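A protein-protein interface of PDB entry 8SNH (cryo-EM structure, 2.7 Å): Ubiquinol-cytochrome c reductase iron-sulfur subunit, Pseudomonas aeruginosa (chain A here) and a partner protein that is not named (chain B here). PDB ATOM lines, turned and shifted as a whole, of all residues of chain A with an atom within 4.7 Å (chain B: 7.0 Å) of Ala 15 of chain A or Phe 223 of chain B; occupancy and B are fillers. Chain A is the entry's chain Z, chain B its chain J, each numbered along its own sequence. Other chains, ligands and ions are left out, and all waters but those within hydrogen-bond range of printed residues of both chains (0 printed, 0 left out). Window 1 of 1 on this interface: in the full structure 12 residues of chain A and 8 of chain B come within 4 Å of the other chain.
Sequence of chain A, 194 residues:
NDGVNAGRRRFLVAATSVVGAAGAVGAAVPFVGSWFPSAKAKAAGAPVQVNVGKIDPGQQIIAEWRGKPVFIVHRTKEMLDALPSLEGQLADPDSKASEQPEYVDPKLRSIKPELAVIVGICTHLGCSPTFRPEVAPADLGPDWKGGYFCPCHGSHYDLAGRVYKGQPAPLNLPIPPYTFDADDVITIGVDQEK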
ATOM      1  N   PHE A  11     -14.238  29.841  -8.881  1.00  0.00           N
ATOM      2  CA  PHE A  11     -13.375  29.768  -7.707  1.00  0.00           C
ATOM      3  C   PHE A  11     -12.087  29.023  -8.016  1.00  0.00           C
ATOM      4  O   PHE A  11     -11.006  29.446  -7.599  1.00  0.00           O
ATOM      5  CB  PHE A  11     -14.088  29.085  -6.543  1.00  0.00           C
ATOM      6  CG  PHE A  11     -13.144  28.578  -5.488  1.00  0.00           C
ATOM      7  CD1 PHE A  11     -12.543  29.456  -4.601  1.00  0.00           C
ATOM      8  CD2 PHE A  11     -12.830  27.232  -5.404  1.00  0.00           C
ATOM      9  CE1 PHE A  11     -11.664  28.998  -3.639  1.00  0.00           C
ATOM     10  CE2 PHE A  11     -11.952  26.769  -4.443  1.00  0.00           C
ATOM     11  CZ  PHE A  11     -11.367  27.654  -3.561  1.00  0.00           C
ATOM     12  N   LEU A  12     -12.183  27.893  -8.718  1.00  0.00           N
ATOM     13  CA  LEU A  12     -10.983  27.127  -9.027  1.00  0.00           C
ATOM     14  C   LEU A  12     -10.053  27.913  -9.941  1.00  0.00           C
ATOM     15  O   LEU A  12      -8.835  27.908  -9.743  1.00  0.00           O
ATOM     16  CB  LEU A  12     -11.355  25.787  -9.661  1.00  0.00           C
ATOM     17  CG  LEU A  12     -11.717  24.671  -8.677  1.00  0.00           C
ATOM     18  CD1 LEU A  12     -12.277  23.467  -9.416  1.00  0.00           C
ATOM     19  CD2 LEU A  12     -10.513  24.273  -7.837  1.00  0.00           C
ATOM     20  N   VAL A  13     -10.606  28.607 -10.935  1.00  0.00           N
ATOM     21  CA  VAL A  13      -9.775  29.412 -11.825  1.00  0.00           C
ATOM     22  C   VAL A  13      -9.076  30.509 -11.034  1.00  0.00           C
ATOM     23  O   VAL A  13      -7.871  30.734 -11.187  1.00  0.00           O
ATOM     24  CB  VAL A  13     -10.622  29.991 -12.971  1.00  0.00           C
ATOM     25  CG1 VAL A  13      -9.868  31.103 -13.685  1.00  0.00           C
ATOM     26  CG2 VAL A  13     -11.007  28.895 -13.948  1.00  0.00           C
ATOM     27  N   ALA A  14      -9.817  31.197 -10.162  1.00  0.00           N
ATOM     28  CA  ALA A  14      -9.226  32.279  -9.382  1.00  0.00           C
ATOM     29  C   ALA A  14      -8.155  31.760  -8.428  1.00  0.00           C
ATOM     30  O   ALA A  14      -7.083  32.361  -8.302  1.00  0.00           O
ATOM     31  CB  ALA A  14     -10.316  33.019  -8.608  1.00  0.00           C
ATOM     32  N   ALA A  15      -8.432  30.653  -7.738  1.00  0.00           N
ATOM     33  CA  ALA A  15      -7.467  30.103  -6.792  1.00  0.00           C
ATOM     34  C   ALA A  15      -6.213  29.617  -7.505  1.00  0.00           C
ATOM     35  O   ALA A  15      -5.093  29.874  -7.045  1.00  0.00           O
ATOM     36  CB  ALA A  15      -8.105  28.964  -5.999  1.00  0.00           C
ATOM     37  N   THR A  16      -6.377  28.911  -8.624  1.00  0.00           N
ATOM     38  CA  THR A  16      -5.222  28.462  -9.387  1.00  0.00           C
ATOM     39  C   THR A  16      -4.428  29.650  -9.912  1.00  0.00           C
ATOM     40  O   THR A  16      -3.196  29.628  -9.902  1.00  0.00           O
ATOM     41  CB  THR A  16      -5.670  27.560 -10.536  1.00  0.00           C
ATOM     42  OG1 THR A  16      -6.639  26.618 -10.059  1.00  0.00           O
ATOM     43  CG2 THR A  16      -4.487  26.806 -11.117  1.00  0.00           C
ATOM     44  N   SER A  17      -5.116  30.702 -10.361  1.00  0.00           N
ATOM     45  CA  SER A  17      -4.420  31.887 -10.847  1.00  0.00           C
ATOM     46  C   SER A  17      -3.633  32.562  -9.733  1.00  0.00           C
ATOM     47  O   SER A  17      -2.489  32.976  -9.938  1.00  0.00           O
ATOM     48  CB  SER A  17      -5.424  32.863 -11.457  1.00  0.00           C
ATOM     49  OG  SER A  17      -6.146  32.255 -12.512  1.00  0.00           O
ATOM     50  N   VAL A  18      -4.226  32.682  -8.545  1.00  0.00           N
ATOM     51  CA  VAL A  18      -3.536  33.332  -7.435  1.00  0.00           C
ATOM     52  C   VAL A  18      -2.332  32.507  -6.996  1.00  0.00           C
ATOM     53  O   VAL A  18      -1.249  33.049  -6.742  1.00  0.00           O
ATOM     54  CB  VAL A  18      -4.513  33.575  -6.271  1.00  0.00           C
ATOM     55  CG1 VAL A  18      -3.755  33.912  -4.997  1.00  0.00           C
ATOM     56  CG2 VAL A  18      -5.489  34.685  -6.625  1.00  0.00           C
ATOM     57  N   VAL A  19      -2.498  31.187  -6.899  1.00  0.00           N
ATOM     58  CA  VAL A  19      -1.385  30.334  -6.498  1.00  0.00           C
ATOM     59  C   VAL A  19      -0.285  30.368  -7.551  1.00  0.00           C
ATOM     60  O   VAL A  19       0.906  30.408  -7.224  1.00  0.00           O
ATOM     61  CB  VAL A  19      -1.885  28.903  -6.231  1.00  0.00           C
ATOM     62  CG1 VAL A  19      -0.719  27.963  -5.992  1.00  0.00           C
ATOM     63  CG2 VAL A  19      -2.828  28.888  -5.037  1.00  0.00           C
ATOM     64  N   LEU B 217       4.588  23.559  -4.551  1.00  0.00           N
ATOM     65  CA  LEU B 217       4.214  22.894  -5.790  1.00  0.00           C
ATOM     66  C   LEU B 217       3.163  21.822  -5.552  1.00  0.00           C
ATOM     67  O   LEU B 217       2.313  21.602  -6.412  1.00  0.00           O
ATOM     68  CB  LEU B 217       5.451  22.302  -6.465  1.00  0.00           C
ATOM     69  CG  LEU B 217       6.307  23.319  -7.229  1.00  0.00           C
ATOM     70  CD1 LEU B 217       7.628  22.711  -7.658  1.00  0.00           C
ATOM     71  CD2 LEU B 217       5.557  23.860  -8.437  1.00  0.00           C
ATOM     72  N   ALA B 218       3.187  21.154  -4.397  1.00  0.00           N
ATOM     73  CA  ALA B 218       2.108  20.227  -4.069  1.00  0.00           C
ATOM     74  C   ALA B 218       0.785  20.966  -3.902  1.00  0.00           C
ATOM     75  O   ALA B 218      -0.257  20.517  -4.397  1.00  0.00           O
ATOM     76  CB  ALA B 218       2.454  19.450  -2.800  1.00  0.00           C
ATOM     77  N   PHE B 219       0.809  22.104  -3.207  1.00  0.00           N
ATOM     78  CA  PHE B 219      -0.391  22.931  -3.075  1.00  0.00           C
ATOM     79  C   PHE B 219      -0.927  23.341  -4.447  1.00  0.00           C
ATOM     80  O   PHE B 219      -2.115  23.151  -4.767  1.00  0.00           O
ATOM     81  CB  PHE B 219      -0.036  24.153  -2.222  1.00  0.00           C
ATOM     82  CG  PHE B 219      -1.210  24.841  -1.586  1.00  0.00           C
ATOM     83  CD1 PHE B 219      -1.608  26.091  -2.022  1.00  0.00           C
ATOM     84  CD2 PHE B 219      -1.894  24.253  -0.535  1.00  0.00           C
ATOM     85  CE1 PHE B 219      -2.671  26.741  -1.431  1.00  0.00           C
ATOM     86  CE2 PHE B 219      -2.965  24.898   0.057  1.00  0.00           C
ATOM     87  CZ  PHE B 219      -3.352  26.145  -0.390  1.00  0.00           C
ATOM     88  N   PHE B 220      -0.045  23.892  -5.281  1.00  0.00           N
ATOM     89  CA  PHE B 220      -0.432  24.327  -6.614  1.00  0.00           C
ATOM     90  C   PHE B 220      -0.919  23.154  -7.452  1.00  0.00           C
ATOM     91  O   PHE B 220      -1.828  23.315  -8.269  1.00  0.00           O
ATOM     92  CB  PHE B 220       0.755  25.011  -7.297  1.00  0.00           C
ATOM     93  CG  PHE B 220       0.436  25.610  -8.642  1.00  0.00           C
ATOM     94  CD1 PHE B 220      -0.871  25.819  -9.050  1.00  0.00           C
ATOM     95  CD2 PHE B 220       1.457  25.937  -9.512  1.00  0.00           C
ATOM     96  CE1 PHE B 220      -1.147  26.362 -10.284  1.00  0.00           C
ATOM     97  CE2 PHE B 220       1.181  26.474 -10.747  1.00  0.00           C
ATOM     98  CZ  PHE B 220      -0.121  26.686 -11.134  1.00  0.00           C
ATOM     99  N   PHE B 221      -0.322  21.972  -7.278  1.00  0.00           N
ATOM    100  CA  PHE B 221      -0.785  20.799  -8.005  1.00  0.00           C
ATOM    101  C   PHE B 221      -2.192  20.424  -7.591  1.00  0.00           C
ATOM    102  O   PHE B 221      -3.005  20.037  -8.430  1.00  0.00           O
ATOM    103  CB  PHE B 221       0.141  19.608  -7.773  1.00  0.00           C
ATOM    104  CG  PHE B 221      -0.412  18.318  -8.308  1.00  0.00           C
ATOM    105  CD1 PHE B 221      -0.304  18.008  -9.652  1.00  0.00           C
ATOM    106  CD2 PHE B 221      -1.071  17.431  -7.475  1.00  0.00           C
ATOM    107  CE1 PHE B 221      -0.822  16.831 -10.150  1.00  0.00           C
ATOM    108  CE2 PHE B 221      -1.591  16.252  -7.969  1.00  0.00           C
ATOM    109  CZ  PHE B 221      -1.466  15.953  -9.308  1.00  0.00           C
ATOM    110  N   VAL B 222      -2.491  20.493  -6.296  1.00  0.00           N
ATOM    111  CA  VAL B 222      -3.852  20.210  -5.854  1.00  0.00           C
ATOM    112  C   VAL B 222      -4.826  21.135  -6.569  1.00  0.00           C
ATOM    113  O   VAL B 222      -5.829  20.695  -7.149  1.00  0.00           O
ATOM    114  CB  VAL B 222      -3.961  20.346  -4.325  1.00  0.00           C
ATOM    115  CG1 VAL B 222      -5.417  20.475  -3.902  1.00  0.00           C
ATOM    116  CG2 VAL B 222      -3.306  19.161  -3.640  1.00  0.00           C
ATOM    117  N   PHE B 223      -4.523  22.434  -6.566  1.00  0.00           N
ATOM    118  CA  PHE B 223      -5.435  23.387  -7.200  1.00  0.00           C
ATOM    119  C   PHE B 223      -5.534  23.172  -8.707  1.00  0.00           C
ATOM    120  O   PHE B 223      -6.632  23.224  -9.273  1.00  0.00           O
ATOM    121  CB  PHE B 223      -5.012  24.812  -6.868  1.00  0.00           C
ATOM    122  CG  PHE B 223      -5.412  25.234  -5.493  1.00  0.00           C
ATOM    123  CD1 PHE B 223      -6.645  25.821  -5.271  1.00  0.00           C
ATOM    124  CD2 PHE B 223      -4.595  24.982  -4.412  1.00  0.00           C
ATOM    125  CE1 PHE B 223      -7.029  26.193  -4.003  1.00  0.00           C
ATOM    126  CE2 PHE B 223      -4.976  25.345  -3.144  1.00  0.00           C
ATOM    127  CZ  PHE B 223      -6.195  25.952  -2.937  1.00  0.00           C
ATOM    128  N   ALA B 224      -4.409  22.922  -9.377  1.00  0.00           N
ATOM    129  CA  ALA B 224      -4.436  22.721 -10.822  1.00  0.00           C
ATOM    130  C   ALA B 224      -5.161  21.432 -11.187  1.00  0.00           C
ATOM    131  O   ALA B 224      -5.896  21.386 -12.175  1.00  0.00           O
ATOM    132  CB  ALA B 224      -3.013  22.708 -11.376  1.00  0.00           C
ATOM    133  N   TYR B 225      -4.961  20.373 -10.402  1.00  0.00           N
ATOM    134  CA  TYR B 225      -5.661  19.121 -10.643  1.00  0.00           C
ATOM    135  C   TYR B 225      -7.162  19.296 -10.480  1.00  0.00           C
ATOM    136  O   TYR B 225      -7.943  18.750 -11.265  1.00  0.00           O
ATOM    137  CB  TYR B 225      -5.142  18.046  -9.691  1.00  0.00           C
ATOM    138  CG  TYR B 225      -5.839  16.715  -9.834  1.00  0.00           C
ATOM    139  CD1 TYR B 225      -5.408  15.779 -10.763  1.00  0.00           C
ATOM    140  CD2 TYR B 225      -6.933  16.395  -9.042  1.00  0.00           C
ATOM    141  CE1 TYR B 225      -6.044  14.562 -10.898  1.00  0.00           C
ATOM    142  CE2 TYR B 225      -7.576  15.181  -9.170  1.00  0.00           C
ATOM    143  CZ  TYR B 225      -7.127  14.268 -10.099  1.00  0.00           C
ATOM    144  OH  TYR B 225      -7.766  13.057 -10.228  1.00  0.00           O
ATOM    145  N   LEU B 226      -7.591  20.036  -9.454  1.00  0.00           N
ATOM    146  CA  LEU B 226      -9.021  20.289  -9.306  1.00  0.00           C
ATOM    147  C   LEU B 226      -9.553  21.124 -10.465  1.00  0.00           C
ATOM    148  O   LEU B 226     -10.624  20.832 -11.007  1.00  0.00           O
ATOM    149  CB  LEU B 226      -9.305  20.978  -7.973  1.00  0.00           C
ATOM    150  CG  LEU B 226      -9.024  20.146  -6.720  1.00  0.00           C
ATOM    151  CD1 LEU B 226      -9.330  20.952  -5.471  1.00  0.00           C
ATOM    152  CD2 LEU B 226      -9.814  18.848  -6.728  1.00  0.00           C
ATOM    153  N   LEU B 227      -8.816  22.163 -10.864  1.00  0.00           N
ATOM    154  CA  LEU B 227      -9.228  22.984 -11.997  1.00  0.00           C
ATOM    155  C   LEU B 227      -9.236  22.201 -13.302  1.00  0.00           C
ATOM    156  O   LEU B 227      -9.915  22.609 -14.248  1.00  0.00           O
ATOM    157  CB  LEU B 227      -8.305  24.198 -12.120  1.00  0.00           C
ATOM    158  CG  LEU B 227      -8.427  25.059 -13.381  1.00  0.00           C
ATOM    159  CD1 LEU B 227      -9.810  25.678 -13.483  1.00  0.00           C
ATOM    160  CD2 LEU B 227      -7.358  26.137 -13.384  1.00  0.00           C
ATOM    161  N   LYS B 228      -8.477  21.109 -13.384  1.00  0.00           N
ATOM    162  CA  LYS B 228      -8.468  20.287 -14.589  1.00  0.00           C
ATOM    163  C   LYS B 228      -9.608  19.277 -14.579  1.00  0.00           C
ATOM    164  O   LYS B 228     -10.422  19.236 -15.506  1.00  0.00           O
ATOM    165  CB  LYS B 228      -7.128  19.563 -14.727  1.00  0.00           C
ATOM    166  CG  LYS B 228      -6.976  18.811 -16.038  1.00  0.00           C
ATOM    167  CD  LYS B 228      -7.342  17.340 -15.903  1.00  0.00           C
ATOM    168  CE  LYS B 228      -7.432  16.664 -17.260  1.00  0.00           C
ATOM    169  NZ  LYS B 228      -8.217  15.402 -17.208  1.00  0.00           N
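Leu 12 of chain A touches Leu 226 of chain B.
Leu 227 of chain B touches Leu 12 of chain A.
CD1 of Leu 227 of chain B touches CG2 of Val 13 of chain A (3.5 Å).
Phe 223 of chain B touches Ala 15 of chain A.
Thr 16 of chain A touches Phe 220 of chain B.
Thr 16 of chain A touches Leu 227 of chain B (OG1 to CD2, 3.4 Å).
Val 19 of chain A touches Phe 220 of chain B (CG1 to CB, 3.5 Å).
The backbone carbonyl oxygen of Val 13 of chain A sits at hydrogen-bond distance from the side-chain hydroxyl of Ser 17 of chain A (2.7 Å).
OG1 of Thr 16 of chain A sits at hydrogen-bond distance from O of Leu 12 of chain A (2.6 Å).
Of the 9 printed residues of chain A, 5 touch a printed residue of chain B.
Hydrophobic or aromatic side chains of chain A that line the printed part of chain B: Leu 12, Val 13, Ala 15 and Val 19.
Hydrophobic or aromatic side chains of chain B that line the printed part of chain A: Phe 220, Phe 223, Leu 226 and Leu 227.
Along chain B the printed residues that touch a printed residue of chain A span positions 220 to 227.
Among the printed residues, 8 pairs touch across the chains.
Among the printed residues, no Asp or Glu carboxylate lies within 4 Å of a Lys or Arg side-chain nitrogen of the other chain.
OG1 of Thr 16 of chain A sits at hydrogen-bond distance from O of Phe 223 of chain B (3.5 Å).
Of chain B, only Phe 223 (3.5 Å) comes within 4 Å of Ala 15 of chain A.
Phe 223 of chain B touches two residues of chain A.
Printed residues of chain B within 4 Å of Leu 12 of chain A: Leu 226 and Leu 227.
Of the printed residues of chain A, Leu 227 of chain B touches Leu 12 (3.97 Å), Val 13 (3.5 Å) and Thr 16 (3.4 Å).
Printed residues of chain A within 4 Å of Leu 226 of chain B: Leu 12 (3.5 Å).
Leu 217 of chain B touches none of the printed residues of chain A.
The nearest residue of chain B that does not touch Ala 15 of chain A is Phe 220 of chain B (6.2 Å).
The nearest printed residue of chain A that does not touch Leu 226 of chain B is Thr 16 of chain A (6.2 Å).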
